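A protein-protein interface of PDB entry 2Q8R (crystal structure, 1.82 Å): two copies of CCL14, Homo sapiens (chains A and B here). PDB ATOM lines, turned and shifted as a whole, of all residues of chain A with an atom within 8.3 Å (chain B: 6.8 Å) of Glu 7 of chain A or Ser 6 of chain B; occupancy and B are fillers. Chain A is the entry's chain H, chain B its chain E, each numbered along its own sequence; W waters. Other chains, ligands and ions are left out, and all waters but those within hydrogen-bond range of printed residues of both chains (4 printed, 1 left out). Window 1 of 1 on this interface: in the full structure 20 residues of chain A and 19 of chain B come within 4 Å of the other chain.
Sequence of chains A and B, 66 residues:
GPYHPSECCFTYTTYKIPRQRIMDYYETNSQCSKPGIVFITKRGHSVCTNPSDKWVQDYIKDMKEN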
ATOM      1  N   HIS A   4     -17.783  10.829  -9.694  1.00  0.00           N
ATOM      2  CA  HIS A   4     -18.495  11.781 -10.550  1.00  0.00           C
ATOM      3  C   HIS A   4     -17.543  12.250 -11.673  1.00  0.00           C
ATOM      4  O   HIS A   4     -16.330  12.359 -11.439  1.00  0.00           O
ATOM      5  CB  HIS A   4     -19.059  12.960  -9.726  1.00  0.00           C
ATOM      6  CG  HIS A   4     -18.012  13.901  -9.202  1.00  0.00           C
ATOM      7  ND1 HIS A   4     -17.509  14.947  -9.950  1.00  0.00           N
ATOM      8  CD2 HIS A   4     -17.391  13.971  -8.001  1.00  0.00           C
ATOM      9  CE1 HIS A   4     -16.596  15.596  -9.248  1.00  0.00           C
ATOM     10  NE2 HIS A   4     -16.511  15.029  -8.055  1.00  0.00           N
ATOM     11  N   PRO A   5     -18.081  12.522 -12.890  1.00  0.00           N
ATOM     12  CA  PRO A   5     -17.259  13.158 -13.934  1.00  0.00           C
ATOM     13  C   PRO A   5     -17.030  14.645 -13.645  1.00  0.00           C
ATOM     14  O   PRO A   5     -17.720  15.220 -12.771  1.00  0.00           O
ATOM     15  CB  PRO A   5     -18.095  12.995 -15.214  1.00  0.00           C
ATOM     16  CG  PRO A   5     -19.551  12.966 -14.692  1.00  0.00           C
ATOM     17  CD  PRO A   5     -19.466  12.263 -13.340  1.00  0.00           C
ATOM     18  N   SER A   6     -16.064  15.253 -14.338  1.00  0.00           N
ATOM     19  CA  SER A   6     -15.807  16.686 -14.210  1.00  0.00           C
ATOM     20  C   SER A   6     -15.974  17.315 -15.569  1.00  0.00           C
ATOM     21  O   SER A   6     -15.639  16.698 -16.599  1.00  0.00           O
ATOM     22  CB  SER A   6     -14.370  16.968 -13.741  1.00  0.00           C
ATOM     23  OG  SER A   6     -14.162  16.473 -12.436  1.00  0.00           O
ATOM     24  N   GLU A   7     -16.470  18.545 -15.566  1.00  0.00           N
ATOM     25  CA  GLU A   7     -16.554  19.330 -16.805  1.00  0.00           C
ATOM     26  C   GLU A   7     -15.153  19.755 -17.249  1.00  0.00           C
ATOM     27  O   GLU A   7     -14.384  20.325 -16.433  1.00  0.00           O
ATOM     28  CB  GLU A   7     -17.397  20.576 -16.587  1.00  0.00           C
ATOM     29  CG  GLU A   7     -18.857  20.302 -16.143  1.00  0.00           C
ATOM     30  CD  GLU A   7     -19.055  20.284 -14.619  1.00  0.00           C
ATOM     31  OE1 GLU A   7     -18.071  20.132 -13.848  1.00  0.00           O
ATOM     32  OE2 GLU A   7     -20.230  20.405 -14.191  1.00  0.00           O
ATOM     33  N   CYS A   8     -14.813  19.460 -18.509  1.00  0.00           N
ATOM     34  CA  CYS A   8     -13.532  19.907 -19.110  1.00  0.00           C
ATOM     35  C   CYS A   8     -13.766  20.656 -20.415  1.00  0.00           C
ATOM     36  O   CYS A   8     -14.733  20.371 -21.137  1.00  0.00           O
ATOM     37  CB  CYS A   8     -12.635  18.709 -19.411  1.00  0.00           C
ATOM     38  SG  CYS A   8     -12.111  17.793 -17.927  1.00  0.00           S
ATOM     39  N   CYS A   9     -12.874  21.594 -20.708  1.00  0.00           N
ATOM     40  CA  CYS A   9     -12.986  22.440 -21.902  1.00  0.00           C
ATOM     41  C   CYS A   9     -12.119  21.928 -23.037  1.00  0.00           C
ATOM     42  O   CYS A   9     -10.951  21.577 -22.831  1.00  0.00           O
ATOM     43  CB  CYS A   9     -12.584  23.886 -21.578  1.00  0.00           C
ATOM     44  SG  CYS A   9     -13.804  24.725 -20.574  1.00  0.00           S
ATOM     45  N   PHE A  10     -12.686  21.897 -24.237  1.00  0.00           N
ATOM     46  CA  PHE A  10     -11.935  21.468 -25.423  1.00  0.00           C
ATOM     47  C   PHE A  10     -11.941  22.513 -26.530  1.00  0.00           C
ATOM     48  O   PHE A  10     -10.903  22.739 -27.174  1.00  0.00           O
ATOM     49  CB  PHE A  10     -12.443  20.126 -25.943  1.00  0.00           C
ATOM     50  CG  PHE A  10     -12.205  19.018 -24.978  1.00  0.00           C
ATOM     51  CD1 PHE A  10     -10.914  18.596 -24.724  1.00  0.00           C
ATOM     52  CD2 PHE A  10     -13.265  18.470 -24.260  1.00  0.00           C
ATOM     53  CE1 PHE A  10     -10.673  17.586 -23.787  1.00  0.00           C
ATOM     54  CE2 PHE A  10     -13.037  17.481 -23.320  1.00  0.00           C
ATOM     55  CZ  PHE A  10     -11.747  17.046 -23.081  1.00  0.00           C
ATOM     56  N   THR A  11     -13.109  23.112 -26.753  1.00  0.00           N
ATOM     57  CA  THR A  11     -13.244  24.222 -27.704  1.00  0.00           C
ATOM     58  C   THR A  11     -13.505  25.525 -26.957  1.00  0.00           C
ATOM     59  O   THR A  11     -14.597  25.730 -26.409  1.00  0.00           O
ATOM     60  CB  THR A  11     -14.383  23.968 -28.698  1.00  0.00           C
ATOM     61  OG1 THR A  11     -14.245  22.654 -29.266  1.00  0.00           O
ATOM     62  CG2 THR A  11     -14.334  25.015 -29.831  1.00  0.00           C
ATOM     63  N   TYR A  26     -16.662  29.204 -13.162  1.00  0.00           N
ATOM     64  CA  TYR A  26     -15.896  28.244 -12.377  1.00  0.00           C
ATOM     65  C   TYR A  26     -14.665  27.854 -13.142  1.00  0.00           C
ATOM     66  O   TYR A  26     -14.660  27.873 -14.388  1.00  0.00           O
ATOM     67  CB  TYR A  26     -16.727  27.018 -11.966  1.00  0.00           C
ATOM     68  CG  TYR A  26     -17.227  26.128 -13.075  1.00  0.00           C
ATOM     69  CD1 TYR A  26     -16.425  25.107 -13.605  1.00  0.00           C
ATOM     70  CD2 TYR A  26     -18.522  26.281 -13.576  1.00  0.00           C
ATOM     71  CE1 TYR A  26     -16.892  24.279 -14.628  1.00  0.00           C
ATOM     72  CE2 TYR A  26     -19.010  25.445 -14.583  1.00  0.00           C
ATOM     73  CZ  TYR A  26     -18.178  24.443 -15.105  1.00  0.00           C
ATOM     74  OH  TYR A  26     -18.669  23.615 -16.097  1.00  0.00           O
ATOM     75  N   GLU A  27     -13.606  27.503 -12.410  1.00  0.00           N
ATOM     76  CA  GLU A  27     -12.420  26.936 -13.050  1.00  0.00           C
ATOM     77  C   GLU A  27     -12.596  25.439 -13.127  1.00  0.00           C
ATOM     78  O   GLU A  27     -12.998  24.809 -12.148  1.00  0.00           O
ATOM     79  CB  GLU A  27     -11.123  27.269 -12.278  1.00  0.00           C
ATOM     80  CG  GLU A  27      -9.833  26.811 -13.034  1.00  0.00           C
ATOM     81  CD  GLU A  27      -8.537  27.216 -12.338  1.00  0.00           C
ATOM     82  OE1 GLU A  27      -8.599  27.795 -11.221  1.00  0.00           O
ATOM     83  OE2 GLU A  27      -7.471  26.920 -12.921  1.00  0.00           O
ATOM     84  N   THR A  28     -12.260  24.866 -14.277  1.00  0.00           N
ATOM     85  CA  THR A  28     -12.430  23.428 -14.445  1.00  0.00           C
ATOM     86  C   THR A  28     -11.393  22.665 -13.615  1.00  0.00           C
ATOM     87  O   THR A  28     -10.332  23.204 -13.257  1.00  0.00           O
ATOM     88  CB  THR A  28     -12.367  23.024 -15.921  1.00  0.00           C
ATOM     89  OG1 THR A  28     -11.196  23.596 -16.537  1.00  0.00           O
ATOM     90  CG2 THR A  28     -13.625  23.543 -16.635  1.00  0.00           C
ATOM     91  N   ASN A  29     -11.711  21.405 -13.326  1.00  0.00           N
ATOM     92  CA  ASN A  29     -10.807  20.493 -12.630  1.00  0.00           C
ATOM     93  C   ASN A  29      -9.392  20.561 -13.221  1.00  0.00           C
ATOM     94  O   ASN A  29      -9.209  20.464 -14.445  1.00  0.00           O
ATOM     95  CB  ASN A  29     -11.398  19.080 -12.770  1.00  0.00           C
ATOM     96  CG  ASN A  29     -10.707  18.041 -11.902  1.00  0.00           C
ATOM     97  OD1 ASN A  29      -9.531  18.141 -11.571  1.00  0.00           O
ATOM     98  ND2 ASN A  29     -11.464  17.018 -11.539  1.00  0.00           N
ATOM     99  N   SER A  30      -8.380  20.779 -12.374  1.00  0.00           N
ATOM    100  CA  SER A  30      -7.008  20.840 -12.900  1.00  0.00           C
ATOM    101  C   SER A  30      -6.544  19.524 -13.555  1.00  0.00           C
ATOM    102  O   SER A  30      -5.527  19.492 -14.280  1.00  0.00           O
ATOM    103  CB  SER A  30      -6.040  21.239 -11.787  1.00  0.00           C
ATOM    104  OG  SER A  30      -6.200  20.361 -10.699  1.00  0.00           O
ATOM    105  N   GLN A  31      -7.298  18.442 -13.353  1.00  0.00           N
ATOM    106  CA  GLN A  31      -7.005  17.192 -14.049  1.00  0.00           C
ATOM    107  C   GLN A  31      -7.412  17.166 -15.532  1.00  0.00           C
ATOM    108  O   GLN A  31      -6.941  16.312 -16.282  1.00  0.00           O
ATOM    109  CB  GLN A  31      -7.627  16.000 -13.301  1.00  0.00           C
ATOM    110  CG  GLN A  31      -7.045  15.805 -11.903  1.00  0.00           C
ATOM    111  CD  GLN A  31      -7.830  14.778 -11.122  1.00  0.00           C
ATOM    112  OE1 GLN A  31      -7.824  13.578 -11.451  1.00  0.00           O
ATOM    113  NE2 GLN A  31      -8.534  15.237 -10.091  1.00  0.00           N
ATOM    114  N   CYS A  32      -8.250  18.118 -15.958  1.00  0.00           N
ATOM    115  CA  CYS A  32      -8.579  18.279 -17.368  1.00  0.00           C
ATOM    116  C   CYS A  32      -7.317  18.490 -18.205  1.00  0.00           C
ATOM    117  O   CYS A  32      -6.348  19.060 -17.722  1.00  0.00           O
ATOM    118  CB  CYS A  32      -9.545  19.466 -17.566  1.00  0.00           C
ATOM    119  SG  CYS A  32     -11.182  19.214 -16.765  1.00  0.00           S
ATOM    120  N   SER A  33      -7.331  18.057 -19.459  1.00  0.00           N
ATOM    121  CA  SER A  33      -6.124  18.138 -20.295  1.00  0.00           C
ATOM    122  C   SER A  33      -5.743  19.589 -20.646  1.00  0.00           C
ATOM    123  O   SER A  33      -4.567  19.890 -20.912  1.00  0.00           O
ATOM    124  CB  SER A  33      -6.290  17.272 -21.555  1.00  0.00           C
ATOM    125  OG  SER A  33      -7.211  17.876 -22.446  1.00  0.00           O
ATOM    126  N   LYS A  34      -6.736  20.486 -20.612  1.00  0.00           N
ATOM    127  CA  LYS A  34      -6.516  21.916 -20.877  1.00  0.00           C
ATOM    128  C   LYS A  34      -7.063  22.756 -19.720  1.00  0.00           C
ATOM    129  O   LYS A  34      -8.075  22.388 -19.120  1.00  0.00           O
ATOM    130  CB  LYS A  34      -7.232  22.360 -22.173  1.00  0.00           C
ATOM    131  CG  LYS A  34      -6.950  21.554 -23.456  1.00  0.00           C
ATOM    132  CD  LYS A  34      -7.482  22.392 -24.653  1.00  0.00           C
ATOM    133  CE  LYS A  34      -8.037  21.565 -25.787  1.00  0.00           C
ATOM    134  NZ  LYS A  34      -8.436  22.478 -26.920  1.00  0.00           N
ATOM    135  N   GLY A  36      -9.149  25.743 -18.091  1.00  0.00           N
ATOM    136  CA  GLY A  36     -10.425  26.295 -18.555  1.00  0.00           C
ATOM    137  C   GLY A  36     -11.071  27.151 -17.500  1.00  0.00           C
ATOM    138  O   GLY A  36     -11.053  26.816 -16.321  1.00  0.00           O
ATOM    139  N   VAL A  38     -14.954  28.403 -17.133  1.00  0.00           N
ATOM    140  CA  VAL A  38     -16.296  28.321 -17.720  1.00  0.00           C
ATOM    141  C   VAL A  38     -17.114  29.484 -17.178  1.00  0.00           C
ATOM    142  O   VAL A  38     -17.299  29.597 -15.954  1.00  0.00           O
ATOM    143  CB  VAL A  38     -16.993  26.971 -17.351  1.00  0.00           C
ATOM    144  CG1 VAL A  38     -18.412  26.942 -17.869  1.00  0.00           C
ATOM    145  CG2 VAL A  38     -16.206  25.784 -17.919  1.00  0.00           C
ATOM    146  N   ILE A  40     -20.800  31.066 -16.920  1.00  0.00           N
ATOM    147  CA  ILE A  40     -22.191  30.641 -16.926  1.00  0.00           C
ATOM    148  C   ILE A  40     -23.031  31.858 -17.260  1.00  0.00           C
ATOM    149  O   ILE A  40     -22.956  32.873 -16.572  1.00  0.00           O
ATOM    150  CB  ILE A  40     -22.624  30.097 -15.571  1.00  0.00           C
ATOM    151  CG1 ILE A  40     -21.778  28.864 -15.189  1.00  0.00           C
ATOM    152  CG2 ILE A  40     -24.105  29.706 -15.612  1.00  0.00           C
ATOM    153  CD1 ILE A  40     -21.909  28.457 -13.731  1.00  0.00           C
ATOM    154  N   SER A  46     -23.027  27.396 -20.795  1.00  0.00           N
ATOM    155  CA  SER A  46     -21.707  27.418 -20.205  1.00  0.00           C
ATOM    156  C   SER A  46     -20.749  27.622 -21.371  1.00  0.00           C
ATOM    157  O   SER A  46     -20.887  26.935 -22.398  1.00  0.00           O
ATOM    158  CB  SER A  46     -21.426  26.075 -19.532  1.00  0.00           C
ATOM    159  OG  SER A  46     -22.241  25.904 -18.390  1.00  0.00           O
ATOM    160  N   CYS A  48     -16.706  27.891 -22.474  1.00  0.00           N
ATOM    161  CA  CYS A  48     -15.313  27.650 -22.131  1.00  0.00           C
ATOM    162  C   CYS A  48     -14.426  28.789 -22.620  1.00  0.00           C
ATOM    163  O   CYS A  48     -14.547  29.230 -23.768  1.00  0.00           O
ATOM    164  CB  CYS A  48     -14.840  26.360 -22.793  1.00  0.00           C
ATOM    165  SG  CYS A  48     -15.372  24.876 -21.927  1.00  0.00           S
ATOM    166  N   HIS B   4     -19.462  24.824 -24.958  1.00  0.00           N
ATOM    167  CA  HIS B   4     -19.741  24.236 -23.658  1.00  0.00           C
ATOM    168  C   HIS B   4     -18.666  23.193 -23.323  1.00  0.00           C
ATOM    169  O   HIS B   4     -18.107  22.585 -24.209  1.00  0.00           O
ATOM    170  CB  HIS B   4     -21.139  23.602 -23.623  1.00  0.00           C
ATOM    171  CG  HIS B   4     -21.275  22.397 -24.496  1.00  0.00           C
ATOM    172  ND1 HIS B   4     -20.910  21.133 -24.081  1.00  0.00           N
ATOM    173  CD2 HIS B   4     -21.736  22.258 -25.765  1.00  0.00           C
ATOM    174  CE1 HIS B   4     -21.123  20.270 -25.060  1.00  0.00           C
ATOM    175  NE2 HIS B   4     -21.626  20.926 -26.094  1.00  0.00           N
ATOM    176  N   PRO B   5     -18.384  22.989 -22.023  1.00  0.00           N
ATOM    177  CA  PRO B   5     -17.461  21.920 -21.628  1.00  0.00           C
ATOM    178  C   PRO B   5     -18.112  20.544 -21.781  1.00  0.00           C
ATOM    179  O   PRO B   5     -19.353  20.438 -21.962  1.00  0.00           O
ATOM    180  CB  PRO B   5     -17.195  22.222 -20.137  1.00  0.00           C
ATOM    181  CG  PRO B   5     -18.467  22.865 -19.665  1.00  0.00           C
ATOM    182  CD  PRO B   5     -18.915  23.728 -20.863  1.00  0.00           C
ATOM    183  N   SER B   6     -17.288  19.502 -21.730  1.00  0.00           N
ATOM    184  CA  SER B   6     -17.778  18.129 -21.775  1.00  0.00           C
ATOM    185  C   SER B   6     -17.417  17.417 -20.482  1.00  0.00           C
ATOM    186  O   SER B   6     -16.339  17.641 -19.957  1.00  0.00           O
ATOM    187  CB  SER B   6     -17.102  17.396 -22.928  1.00  0.00           C
ATOM    188  OG  SER B   6     -17.557  17.900 -24.183  1.00  0.00           O
ATOM    189  N   GLU B   7     -18.299  16.535 -20.008  1.00  0.00           N
ATOM    190  CA  GLU B   7     -18.016  15.718 -18.827  1.00  0.00           C
ATOM    191  C   GLU B   7     -16.985  14.662 -19.175  1.00  0.00           C
ATOM    192  O   GLU B   7     -17.146  13.941 -20.176  1.00  0.00           O
ATOM    193  CB  GLU B   7     -19.284  14.998 -18.354  1.00  0.00           C
ATOM    194  CG  GLU B   7     -20.429  15.919 -18.055  1.00  0.00           C
ATOM    195  CD  GLU B   7     -20.251  16.717 -16.790  1.00  0.00           C
ATOM    196  OE1 GLU B   7     -19.295  16.474 -16.010  1.00  0.00           O
ATOM    197  OE2 GLU B   7     -21.093  17.623 -16.574  1.00  0.00           O
ATOM    198  N   CYS B   8     -15.949  14.566 -18.343  1.00  0.00           N
ATOM    199  CA  CYS B   8     -14.909  13.540 -18.501  1.00  0.00           C
ATOM    200  C   CYS B   8     -14.766  12.732 -17.215  1.00  0.00           C
ATOM    201  O   CYS B   8     -14.963  13.261 -16.100  1.00  0.00           O
ATOM    202  CB  CYS B   8     -13.562  14.180 -18.846  1.00  0.00           C
ATOM    203  SG  CYS B   8     -13.528  14.998 -20.480  1.00  0.00           S
ATOM    204  N   PHE B  10     -12.309  10.567 -14.653  1.00  0.00           N
ATOM    205  CA  PHE B  10     -10.911  10.412 -14.216  1.00  0.00           C
ATOM    206  C   PHE B  10     -10.696   9.169 -13.380  1.00  0.00           C
ATOM    207  O   PHE B  10      -9.620   8.582 -13.424  1.00  0.00           O
ATOM    208  CB  PHE B  10     -10.437  11.644 -13.467  1.00  0.00           C
ATOM    209  CG  PHE B  10     -10.365  12.835 -14.352  1.00  0.00           C
ATOM    210  CD1 PHE B  10      -9.438  12.869 -15.389  1.00  0.00           C
ATOM    211  CD2 PHE B  10     -11.298  13.856 -14.236  1.00  0.00           C
ATOM    212  CE1 PHE B  10      -9.389  13.942 -16.253  1.00  0.00           C
ATOM    213  CE2 PHE B  10     -11.258  14.942 -15.109  1.00  0.00           C
ATOM    214  CZ  PHE B  10     -10.318  14.974 -16.117  1.00  0.00           C
ATOM    215  N   THR B  28     -18.950   9.395 -22.677  1.00  0.00           N
ATOM    216  CA  THR B  28     -18.223  10.664 -22.625  1.00  0.00           C
ATOM    217  C   THR B  28     -17.501  10.981 -23.936  1.00  0.00           C
ATOM    218  O   THR B  28     -17.105  10.073 -24.687  1.00  0.00           O
ATOM    219  CB  THR B  28     -17.210  10.716 -21.468  1.00  0.00           C
ATOM    220  OG1 THR B  28     -16.288   9.616 -21.601  1.00  0.00           O
ATOM    221  CG2 THR B  28     -17.959  10.631 -20.124  1.00  0.00           C
ATOM    222  N   ASN B  29     -17.332  12.282 -24.177  1.00  0.00           N
ATOM    223  CA  ASN B  29     -16.645  12.829 -25.352  1.00  0.00           C
ATOM    224  C   ASN B  29     -15.317  12.109 -25.599  1.00  0.00           C
ATOM    225  O   ASN B  29     -14.516  11.931 -24.694  1.00  0.00           O
ATOM    226  CB  ASN B  29     -16.415  14.334 -25.097  1.00  0.00           C
ATOM    227  CG  ASN B  29     -15.785  15.094 -26.286  1.00  0.00           C
ATOM    228  OD1 ASN B  29     -15.226  14.524 -27.226  1.00  0.00           O
ATOM    229  ND2 ASN B  29     -15.852  16.421 -26.199  1.00  0.00           N
ATOM    230  N   GLN B  31     -12.799  13.221 -26.808  1.00  0.00           N
ATOM    231  CA  GLN B  31     -11.676  14.111 -26.497  1.00  0.00           C
ATOM    232  C   GLN B  31     -11.157  13.987 -25.055  1.00  0.00           C
ATOM    233  O   GLN B  31     -10.049  14.441 -24.745  1.00  0.00           O
ATOM    234  CB  GLN B  31     -12.038  15.556 -26.790  1.00  0.00           C
ATOM    235  CG  GLN B  31     -12.229  15.835 -28.299  1.00  0.00           C
ATOM    236  CD  GLN B  31     -12.734  17.241 -28.561  1.00  0.00           C
ATOM    237  OE1 GLN B  31     -13.923  17.540 -28.399  1.00  0.00           O
ATOM    238  NE2 GLN B  31     -11.840  18.109 -28.955  1.00  0.00           N
ATOM    239  N   CYS B  32     -11.960  13.391 -24.175  1.00  0.00           N
ATOM    240  CA  CYS B  32     -11.523  13.108 -22.806  1.00  0.00           C
ATOM    241  C   CYS B  32     -10.292  12.196 -22.825  1.00  0.00           C
ATOM    242  O   CYS B  32     -10.119  11.395 -23.739  1.00  0.00           O
ATOM    243  CB  CYS B  32     -12.655  12.460 -21.982  1.00  0.00           C
ATOM    244  SG  CYS B  32     -14.124  13.535 -21.775  1.00  0.00           S
HETATM  245  O   HOH W   1      -8.414  15.090 -22.824  1.00  0.00           O
HETATM  246  O   HOH W   2     -14.384  10.574 -12.427  1.00  0.00           O
HETATM  247  O   HOH W   3     -15.566  20.069 -27.971  1.00  0.00           O
HETATM  248  O   HOH W   4     -15.389  22.849 -24.899  1.00  0.00           O
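Pro 5 of chain A touches Glu 7 of chain B, and with the chains exchanged Glu 7 of chain A touches Pro 5 of chain B.
Ser 6 of chain A touches its own counterpart, Ser 6 of chain B.
Ser 6 of chain A touches Glu 7 of chain B, and with the chains exchanged Glu 7 of chain A touches Ser 6 of chain B.
Ser 6 of chain A touches Phe 10 of chain B, but with the chains exchanged Phe 10 of chain A does not touch Ser 6 of chain B (4.1 Å).
10 positions are printed for both chains.
Water W1 lies within hydrogen-bond range of O of Gln 31 of chain B (2.6 Å) and OG of Ser 33 of chain A (3.1 Å).
Water W4 lies within hydrogen-bond range of the backbone carbonyl oxygen of His 4 of chain B (2.8 Å), the backbone NH of Phe 10 of chain A (2.9 Å), the backbone NH of Thr 11 of chain A (3.0 Å) and the side-chain sulfur of Cys 48 of chain A (3.6 Å).
Water W2 lies within hydrogen-bond range of the backbone carbonyl oxygen of His 4 of chain A (2.8 Å) and the backbone NH of Phe 10 of chain B (3.0 Å).
Water W3 lies within hydrogen-bond range of the side-chain amide oxygen (OE1) of Gln 31 of chain B (3.0 Å) and the side-chain hydroxyl (OG1) of Thr 11 of chain A (3.2 Å).
Hydrophobic or aromatic side chains of chain B that line the printed part of chain A: His 4, Pro 5 and Phe 10.
Along chain B the printed residues that touch a printed residue of chain A span positions 4 to 32.
Of the 22 printed residues of chain A, 10 touch a printed residue of chain B.
Printed residues of chain A that touch a printed residue of chain B: Pro 5, Ser 6, Glu 7, Cys 8, Phe 10, Tyr 26, Gln 31, Cys 32, Ser 46 and Cys 48.
Hydrophobic or aromatic side chains of chain A that line the printed part of chain B: Pro 5, Phe 10 and Tyr 26.
The backbone carbonyl oxygen (O) of Phe 10 of chain A sits at hydrogen-bond distance from the side-chain amino group (NZ) of Lys 34 of chain A (2.5 Å).
SG of Cys 8 of chain B forms a disulfide with SG of Cys 32 of chain B (2.0 Å).
The side-chain sulfur (SG) of Cys 8 of chain A is disulfide-bonded to the side-chain sulfur (SG) of Cys 32 of chain A, 2.1 Å away.
OG of Ser 6 of chain B sits at hydrogen-bond distance from ND2 of Asn 29 of chain B (3.0 Å).
The backbone NH (N) of Val 38 of chain A sits at hydrogen-bond distance from the backbone carbonyl oxygen (O) of Tyr 26 of chain A, at 2.8 Å.
OD1 of Asn 29 of chain B is in hydrogen-bond range of N of Gln 31 of chain B (2.8 Å).
Among the printed residues, merely in contact across the chains: Pro 5 of chain A with Cys 8 of chain B, Cys 8 of chain A with Pro 5 of chain B, Ser 46 of chain A with His 4 of chain B, Phe 10 of chain A with Gln 31 of chain B, Ser 6 of chain A with Glu 7 of chain B, Gln 31 of chain A with Phe 10 of chain B, Glu 7 of chain A with Glu 7 of chain B, Ser 6 of chain A with Ser 6 of chain B, Glu 7 of chain A with Ser 6 of chain B, Tyr 26 of chain A with Pro 5 of chain B, Ser 46 of chain A with Pro 5 of chain B, Pro 5 of chain A with Glu 7 of chain B, Phe 10 of chain A with Cys 8 of chain B, Cys 32 of chain A with Phe 10 of chain B, Cys 8 of chain A with Phe 10 of chain B, Phe 10 of chain A with Cys 32 of chain B, Phe 10 of chain A with Asn 29 of chain B, Glu 7 of chain A with Pro 5 of chain B, Cys 48 of chain A with His 4 of chain B, Ser 6 of chain A with Phe 10 of chain B and Cys 8 of chain A with Cys 8 of chain B.
Glu 7 of chain A touches just these residues of chain B: Pro 5, Ser 6 and Glu 7.
Printed residues of chain B within 4 Å of Phe 10 of chain A: Cys 8 (3.8 Å), Asn 29 (3.8 Å), Gln 31 (3.3 Å) and Cys 32 (3.8 Å).
Thr 28 of chain A touches none of the printed residues of chain B.
Ile 40 of chain A touches none of the printed residues of chain B.
Ser 6 of chain B touches just these residues of chain A: Ser 6 (3.6 Å), Glu 7 (3.6 Å) and Cys 8 (2.8 Å).
Of the printed residues of chain A, Glu 7 of chain B touches Pro 5 (3.8 Å), Ser 6 (3.4 Å) and Glu 7 (3.5 Å).
Of the printed residues of chain A, Cys 8 of chain B touches Pro 5 (3.2 Å), Ser 6 (2.8 Å), Cys 8 (3.96 Å) and Phe 10 (3.8 Å).
O of Cys 8 of chain A sits at hydrogen-bond distance from N of Ser 6 of chain B, at 2.8 Å.
SG of Cys 48 of chain A lies close to N of Pro 5 of chain B (3.6 Å).
The backbone NH (N) of Cys 8 of chain B is in hydrogen-bond range of the backbone carbonyl oxygen (O) of Ser 6 of chain A (2.8 Å).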
